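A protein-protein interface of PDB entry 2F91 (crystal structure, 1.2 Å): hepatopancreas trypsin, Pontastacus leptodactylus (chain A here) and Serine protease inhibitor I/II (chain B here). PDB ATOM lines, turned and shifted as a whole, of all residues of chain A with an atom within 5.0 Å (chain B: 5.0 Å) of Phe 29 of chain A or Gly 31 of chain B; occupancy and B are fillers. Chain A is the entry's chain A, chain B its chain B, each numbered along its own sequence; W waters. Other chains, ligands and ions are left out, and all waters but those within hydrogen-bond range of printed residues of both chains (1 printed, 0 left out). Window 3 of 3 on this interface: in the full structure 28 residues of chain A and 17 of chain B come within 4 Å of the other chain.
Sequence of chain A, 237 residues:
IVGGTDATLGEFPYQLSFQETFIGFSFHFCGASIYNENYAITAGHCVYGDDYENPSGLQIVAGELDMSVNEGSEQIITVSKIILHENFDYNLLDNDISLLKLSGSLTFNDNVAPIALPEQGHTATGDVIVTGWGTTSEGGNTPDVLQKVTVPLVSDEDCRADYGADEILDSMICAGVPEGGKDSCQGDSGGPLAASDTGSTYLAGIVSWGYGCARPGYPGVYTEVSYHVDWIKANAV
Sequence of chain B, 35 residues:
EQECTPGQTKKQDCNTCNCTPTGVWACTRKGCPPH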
ATOM      1  N   PHE A  18     -24.247   5.350  18.841  1.00  0.00           N
ATOM      2  CA  PHE A  18     -24.466   4.082  19.533  1.00  0.00           C
ATOM      3  C   PHE A  18     -25.941   4.044  19.942  1.00  0.00           C
ATOM      4  O   PHE A  18     -26.400   4.907  20.720  1.00  0.00           O
ATOM      5  CB  PHE A  18     -23.503   3.992  20.699  1.00  0.00           C
ATOM      6  CG  PHE A  18     -23.381   2.657  21.430  1.00  0.00           C
ATOM      7  CD1 PHE A  18     -23.934   1.491  20.932  1.00  0.00           C
ATOM      8  CD2 PHE A  18     -22.653   2.648  22.618  1.00  0.00           C
ATOM      9  CE1 PHE A  18     -23.767   0.310  21.624  1.00  0.00           C
ATOM     10  CE2 PHE A  18     -22.534   1.460  23.330  1.00  0.00           C
ATOM     11  CZ  PHE A  18     -23.092   0.294  22.832  1.00  0.00           C
ATOM     12  N   GLN A  19     -26.670   3.073  19.380  1.00  0.00           N
ATOM     13  CA  GLN A  19     -28.107   2.997  19.472  1.00  0.00           C
ATOM     14  C   GLN A  19     -28.627   1.691  20.047  1.00  0.00           C
ATOM     15  O   GLN A  19     -28.024   0.629  19.900  1.00  0.00           O
ATOM     16  CB  GLN A  19     -28.733   3.178  18.069  1.00  0.00           C
ATOM     17  CG  GLN A  19     -28.295   4.495  17.440  1.00  0.00           C
ATOM     18  CD  GLN A  19     -28.867   4.711  16.064  1.00  0.00           C
ATOM     19  OE1 GLN A  19     -29.580   3.917  15.479  1.00  0.00           O
ATOM     20  NE2 GLN A  19     -28.530   5.881  15.542  1.00  0.00           N
ATOM     21  N   GLU A  20     -29.765   1.796  20.698  1.00  0.00           N
ATOM     22  CA  GLU A  20     -30.483   0.599  21.176  1.00  0.00           C
ATOM     23  C   GLU A  20     -31.820   0.550  20.456  1.00  0.00           C
ATOM     24  O   GLU A  20     -32.479   1.588  20.268  1.00  0.00           O
ATOM     25  CB  GLU A  20     -30.608   0.587  22.679  1.00  0.00           C
ATOM     26  CG  GLU A  20     -31.218   1.802  23.301  1.00  0.00           C
ATOM     27  CD  GLU A  20     -30.838   2.067  24.740  1.00  0.00           C
ATOM     28  OE1 GLU A  20     -29.982   1.364  25.321  1.00  0.00           O
ATOM     29  OE2 GLU A  20     -31.434   3.008  25.319  1.00  0.00           O
ATOM     30  N   PHE A  27     -32.893   4.122  19.224  1.00  0.00           N
ATOM     31  CA  PHE A  27     -32.637   5.223  20.118  1.00  0.00           C
ATOM     32  C   PHE A  27     -31.146   5.464  20.325  1.00  0.00           C
ATOM     33  O   PHE A  27     -30.451   4.612  20.867  1.00  0.00           O
ATOM     34  CB  PHE A  27     -33.310   4.977  21.459  1.00  0.00           C
ATOM     35  CG  PHE A  27     -33.099   6.098  22.460  1.00  0.00           C
ATOM     36  CD1 PHE A  27     -33.747   7.310  22.295  1.00  0.00           C
ATOM     37  CD2 PHE A  27     -32.250   5.945  23.554  1.00  0.00           C
ATOM     38  CE1 PHE A  27     -33.515   8.324  23.229  1.00  0.00           C
ATOM     39  CE2 PHE A  27     -32.016   6.936  24.459  1.00  0.00           C
ATOM     40  CZ  PHE A  27     -32.653   8.155  24.295  1.00  0.00           C
ATOM     41  N   HIS A  28     -30.711   6.643  19.893  1.00  0.00           N
ATOM     42  CA  HIS A  28     -29.356   7.097  20.222  1.00  0.00           C
ATOM     43  C   HIS A  28     -29.213   7.317  21.706  1.00  0.00           C
ATOM     44  O   HIS A  28     -29.883   8.198  22.241  1.00  0.00           O
ATOM     45  CB  HIS A  28     -29.078   8.428  19.469  1.00  0.00           C
ATOM     46  CG  HIS A  28     -27.761   9.026  19.853  1.00  0.00           C
ATOM     47  ND1 HIS A  28     -26.578   8.752  19.162  1.00  0.00           N
ATOM     48  CD2 HIS A  28     -27.439   9.860  20.855  1.00  0.00           C
ATOM     49  CE1 HIS A  28     -25.595   9.410  19.745  1.00  0.00           C
ATOM     50  NE2 HIS A  28     -26.107  10.069  20.795  1.00  0.00           N
ATOM     51  N   PHE A  29     -28.246   6.641  22.344  1.00  0.00           N
ATOM     52  CA  PHE A  29     -28.025   6.922  23.776  1.00  0.00           C
ATOM     53  C   PHE A  29     -26.578   7.286  24.097  1.00  0.00           C
ATOM     54  O   PHE A  29     -26.315   7.773  25.197  1.00  0.00           O
ATOM     55  CB  PHE A  29     -28.443   5.718  24.618  1.00  0.00           C
ATOM     56  CG  PHE A  29     -27.619   4.461  24.414  1.00  0.00           C
ATOM     57  CD1 PHE A  29     -26.527   4.198  25.252  1.00  0.00           C
ATOM     58  CD2 PHE A  29     -27.909   3.552  23.399  1.00  0.00           C
ATOM     59  CE1 PHE A  29     -25.769   3.080  25.009  1.00  0.00           C
ATOM     60  CE2 PHE A  29     -27.139   2.438  23.148  1.00  0.00           C
ATOM     61  CZ  PHE A  29     -26.042   2.202  23.968  1.00  0.00           C
ATOM     62  N   CYS A  30     -25.623   7.069  23.217  1.00  0.00           N
ATOM     63  CA  CYS A  30     -24.203   7.321  23.478  1.00  0.00           C
ATOM     64  C   CYS A  30     -23.539   7.603  22.123  1.00  0.00           C
ATOM     65  O   CYS A  30     -24.065   7.194  21.074  1.00  0.00           O
ATOM     66  CB  CYS A  30     -23.499   6.128  24.176  1.00  0.00           C
ATOM     67  SG  CYS A  30     -23.609   6.193  26.001  1.00  0.00           S
ATOM     68  N   GLY A  31     -22.382   8.227  22.134  1.00  0.00           N
ATOM     69  CA  GLY A  31     -21.485   8.248  20.991  1.00  0.00           C
ATOM     70  C   GLY A  31     -20.463   7.132  21.077  1.00  0.00           C
ATOM     71  O   GLY A  31     -20.355   6.424  22.081  1.00  0.00           O
ATOM     72  N   CYS A  46     -21.448   3.431  29.190  1.00  0.00           N
ATOM     73  CA  CYS A  46     -22.404   3.233  28.121  1.00  0.00           C
ATOM     74  C   CYS A  46     -22.787   1.761  27.992  1.00  0.00           C
ATOM     75  O   CYS A  46     -23.788   1.521  27.338  1.00  0.00           O
ATOM     76  CB  CYS A  46     -21.866   3.746  26.796  1.00  0.00           C
ATOM     77  SG  CYS A  46     -21.766   5.554  26.679  1.00  0.00           S
ATOM     78  N   LEU A  58     -28.264  -3.854  20.156  1.00  0.00           N
ATOM     79  CA  LEU A  58     -27.309  -2.725  20.165  1.00  0.00           C
ATOM     80  C   LEU A  58     -26.660  -2.623  18.789  1.00  0.00           C
ATOM     81  O   LEU A  58     -26.302  -3.626  18.190  1.00  0.00           O
ATOM     82  CB  LEU A  58     -26.232  -2.926  21.197  1.00  0.00           C
ATOM     83  CG  LEU A  58     -26.718  -2.928  22.648  1.00  0.00           C
ATOM     84  CD1 LEU A  58     -25.592  -3.394  23.552  1.00  0.00           C
ATOM     85  CD2 LEU A  58     -27.246  -1.569  23.044  1.00  0.00           C
ATOM     86  N   GLN A 186     -25.718  15.311  28.027  1.00  0.00           N
ATOM     87  CA  GLN A 186     -26.392  14.029  27.990  1.00  0.00           C
ATOM     88  C   GLN A 186     -26.676  13.587  26.549  1.00  0.00           C
ATOM     89  O   GLN A 186     -27.293  14.303  25.775  1.00  0.00           O
ATOM     90  CB  GLN A 186     -27.664  14.086  28.828  1.00  0.00           C
ATOM     91  CG  GLN A 186     -27.430  13.815  30.294  1.00  0.00           C
ATOM     92  CD  GLN A 186     -26.605  14.824  31.060  1.00  0.00           C
ATOM     93  OE1 GLN A 186     -26.852  16.031  30.847  1.00  0.00           O
ATOM     94  NE2 GLN A 186     -25.662  14.451  31.945  1.00  0.00           N
ATOM     95  N   GLY A 187     -26.249  12.392  26.182  1.00  0.00           N
ATOM     96  CA  GLY A 187     -26.274  11.842  24.854  1.00  0.00           C
ATOM     97  C   GLY A 187     -24.952  11.921  24.128  1.00  0.00           C
ATOM     98  O   GLY A 187     -24.806  11.349  23.065  1.00  0.00           O
ATOM     99  N   CYS B  14     -31.592   8.025  33.606  1.00  0.00           N
ATOM    100  CA  CYS B  14     -30.843   6.816  33.306  1.00  0.00           C
ATOM    101  C   CYS B  14     -29.364   6.971  33.648  1.00  0.00           C
ATOM    102  O   CYS B  14     -28.627   5.994  33.532  1.00  0.00           O
ATOM    103  CB  CYS B  14     -30.982   6.487  31.830  1.00  0.00           C
ATOM    104  SG  CYS B  14     -30.096   7.475  30.634  1.00  0.00           S
ATOM    105  N   ASN B  15     -28.947   8.148  34.041  1.00  0.00           N
ATOM    106  CA  ASN B  15     -27.542   8.417  34.361  1.00  0.00           C
ATOM    107  C   ASN B  15     -27.277   8.168  35.835  1.00  0.00           C
ATOM    108  O   ASN B  15     -28.168   8.215  36.715  1.00  0.00           O
ATOM    109  CB  ASN B  15     -27.171   9.845  33.915  1.00  0.00           C
ATOM    110  CG  ASN B  15     -26.924   9.869  32.440  1.00  0.00           C
ATOM    111  OD1 ASN B  15     -26.036   9.176  31.945  1.00  0.00           O
ATOM    112  ND2 ASN B  15     -27.743  10.628  31.717  1.00  0.00           N
ATOM    113  N   ARG B  29     -23.163  11.047  31.138  1.00  0.00           N
ATOM    114  CA  ARG B  29     -23.682  11.807  30.027  1.00  0.00           C
ATOM    115  C   ARG B  29     -24.345  10.949  28.938  1.00  0.00           C
ATOM    116  O   ARG B  29     -24.295  11.227  27.731  1.00  0.00           O
ATOM    117  CB  ARG B  29     -22.598  12.844  29.572  1.00  0.00           C
ATOM    118  CG  ARG B  29     -22.382  13.928  30.488  1.00  0.00           C
ATOM    119  CD  ARG B  29     -21.195  14.776  30.023  1.00  0.00           C
ATOM    120  NE  ARG B  29     -21.209  15.932  30.932  1.00  0.00           N
ATOM    121  CZ  ARG B  29     -20.485  17.012  30.759  1.00  0.00           C
ATOM    122  NH1 ARG B  29     -19.559  17.049  29.836  1.00  0.00           N
ATOM    123  NH2 ARG B  29     -20.631  18.088  31.512  1.00  0.00           N
ATOM    124  N   LYS B  30     -25.033   9.876  29.385  1.00  0.00           N
ATOM    125  CA  LYS B  30     -25.875   9.147  28.403  1.00  0.00           C
ATOM    126  C   LYS B  30     -27.190   9.904  28.012  1.00  0.00           C
ATOM    127  O   LYS B  30     -27.657  10.686  28.862  1.00  0.00           O
ATOM    128  CB  LYS B  30     -26.221   7.778  28.992  1.00  0.00           C
ATOM    129  CG  LYS B  30     -25.157   6.875  29.424  1.00  0.00           C
ATOM    130  CD  LYS B  30     -25.640   5.538  30.065  1.00  0.00           C
ATOM    131  CE  LYS B  30     -26.578   5.792  31.196  1.00  0.00           C
ATOM    132  NZ  LYS B  30     -26.867   4.347  31.668  1.00  0.00           N
ATOM    133  N   GLY B  31     -27.693   9.516  26.867  1.00  0.00           N
ATOM    134  CA  GLY B  31     -29.048  10.004  26.520  1.00  0.00           C
ATOM    135  C   GLY B  31     -30.101   8.993  27.060  1.00  0.00           C
ATOM    136  O   GLY B  31     -29.853   7.846  27.156  1.00  0.00           O
ATOM    137  N   CYS B  32     -31.156   9.618  27.553  1.00  0.00           N
ATOM    138  CA  CYS B  32     -32.174   8.778  28.183  1.00  0.00           C
ATOM    139  C   CYS B  32     -33.503   8.796  27.430  1.00  0.00           C
ATOM    140  O   CYS B  32     -33.989   9.885  27.186  1.00  0.00           O
ATOM    141  CB  CYS B  32     -32.441   9.194  29.622  1.00  0.00           C
ATOM    142  SG  CYS B  32     -30.947   9.329  30.618  1.00  0.00           S
ATOM    143  N   PRO B  33     -34.047   7.645  27.086  1.00  0.00           N
ATOM    144  CA  PRO B  33     -35.296   7.670  26.304  1.00  0.00           C
ATOM    145  C   PRO B  33     -36.475   8.415  26.920  1.00  0.00           C
ATOM    146  O   PRO B  33     -37.381   8.680  26.083  1.00  0.00           O
ATOM    147  CB  PRO B  33     -35.632   6.181  26.115  1.00  0.00           C
ATOM    148  CG  PRO B  33     -34.335   5.465  26.275  1.00  0.00           C
ATOM    149  CD  PRO B  33     -33.558   6.263  27.294  1.00  0.00           C
HETATM  150  O   HOH W   1     -23.168  15.871  33.241  1.00  0.00           O
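The backbone carbonyl oxygen of Phe 29 of chain A sits at hydrogen-bond distance from the backbone NH of Gly 31 of chain B. The backbone NH of Gly 187 of chain A sits close to the backbone NH of Gly 31 of chain B, 3.3 Å away. The backbone NH (N) of Gly 187 of chain A sits close to the backbone carbonyl oxygen (O) of Lys 30 of chain B, 3.5 Å away. The backbone NH (N) of Gly 187 of chain A is in hydrogen-bond range of the backbone carbonyl oxygen (O) of Arg 29 of chain B, at 2.8 Å.
The side-chain amide nitrogen (ND2) of Asn 15 of chain B is in hydrogen-bond range of the side-chain sulfur (SG) of Cys 32 of chain B (3.6 Å). O of Phe 18 of chain A is in hydrogen-bond range of N of Phe 29 of chain A, 3.0 Å away. The backbone NH (N) of Phe 18 of chain A sits at hydrogen-bond distance from the backbone carbonyl oxygen (O) of Cys 30 of chain A, 2.9 Å away. The side-chain amide oxygen of Asn 15 of chain B sits at hydrogen-bond distance from the backbone NH of Lys 30 of chain B (2.8 Å). SG of Cys 30 of chain A forms a disulfide with SG of Cys 46 of chain A. A ring nitrogen (NE2) of His 28 of chain A lies within hydrogen-bond range of the backbone carbonyl oxygen of Gly 187 of chain A (2.9 Å).
Among the printed residues, merely in contact across the chains: Phe 27 of chain A with Pro 33 of chain B (3.2 Å), Phe 27 of chain A with Cys 32 of chain B (3.3 Å), Gln 186 of chain A with Lys 30 of chain B (3.4 Å), Gln 186 of chain A with Asn 15 of chain B (3.5 Å), Gln 186 of chain A with Arg 29 of chain B (3.5 Å), Phe 29 of chain A with Lys 30 of chain B (3.5 Å), Phe 27 of chain A with Gly 31 of chain B (3.6 Å), Cys 30 of chain A with Lys 30 of chain B (3.8 Å) and Glu 20 of chain A with Pro 33 of chain B (3.9 Å).
Gln 19 of chain A touches none of the printed residues of chain B. Phe 29 of chain A touches two residues of chain B. Of the printed residues of chain B, Cys 30 of chain A touches Lys 30. Of the printed residues of chain A, Lys 30 of chain B touches Phe 29 (3.5 Å), Cys 30 (3.8 Å), Gln 186 (3.4 Å) and Gly 187 (3.2 Å). Of chain A, only Phe 27 (3.6 Å), Phe 29 (2.8 Å) and Gly 187 (3.3 Å) come within 4 Å of Gly 31 of chain B. Of the printed residues of chain A, Cys 32 of chain B touches Phe 27 (3.3 Å). The nearest residue of chain B that does not touch Phe 29 of chain A is Arg 29 of chain B (4.7 Å). The nearest printed residue of chain A that does not touch Cys 32 of chain B is Phe 29 of chain A (5.6 Å).
Of the 12 printed residues of chain A, 6 touch a printed residue of chain B. Hydrophobic or aromatic side chains of chain A that line the printed part of chain B: Phe 27 and Phe 29. Along chain A the printed residues that touch a printed residue of chain B span positions 20 to 187. Among the printed residues, 13 pairs touch across the chains. Among the printed residues, no Asp or Glu carboxylate lies within 4 Å of a Lys or Arg side-chain nitrogen of the other chain.
Water W1 bridges NE of Arg 29 of chain B (3.0 Å) and NE2 of Gln 186 of chain A (3.1 Å).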
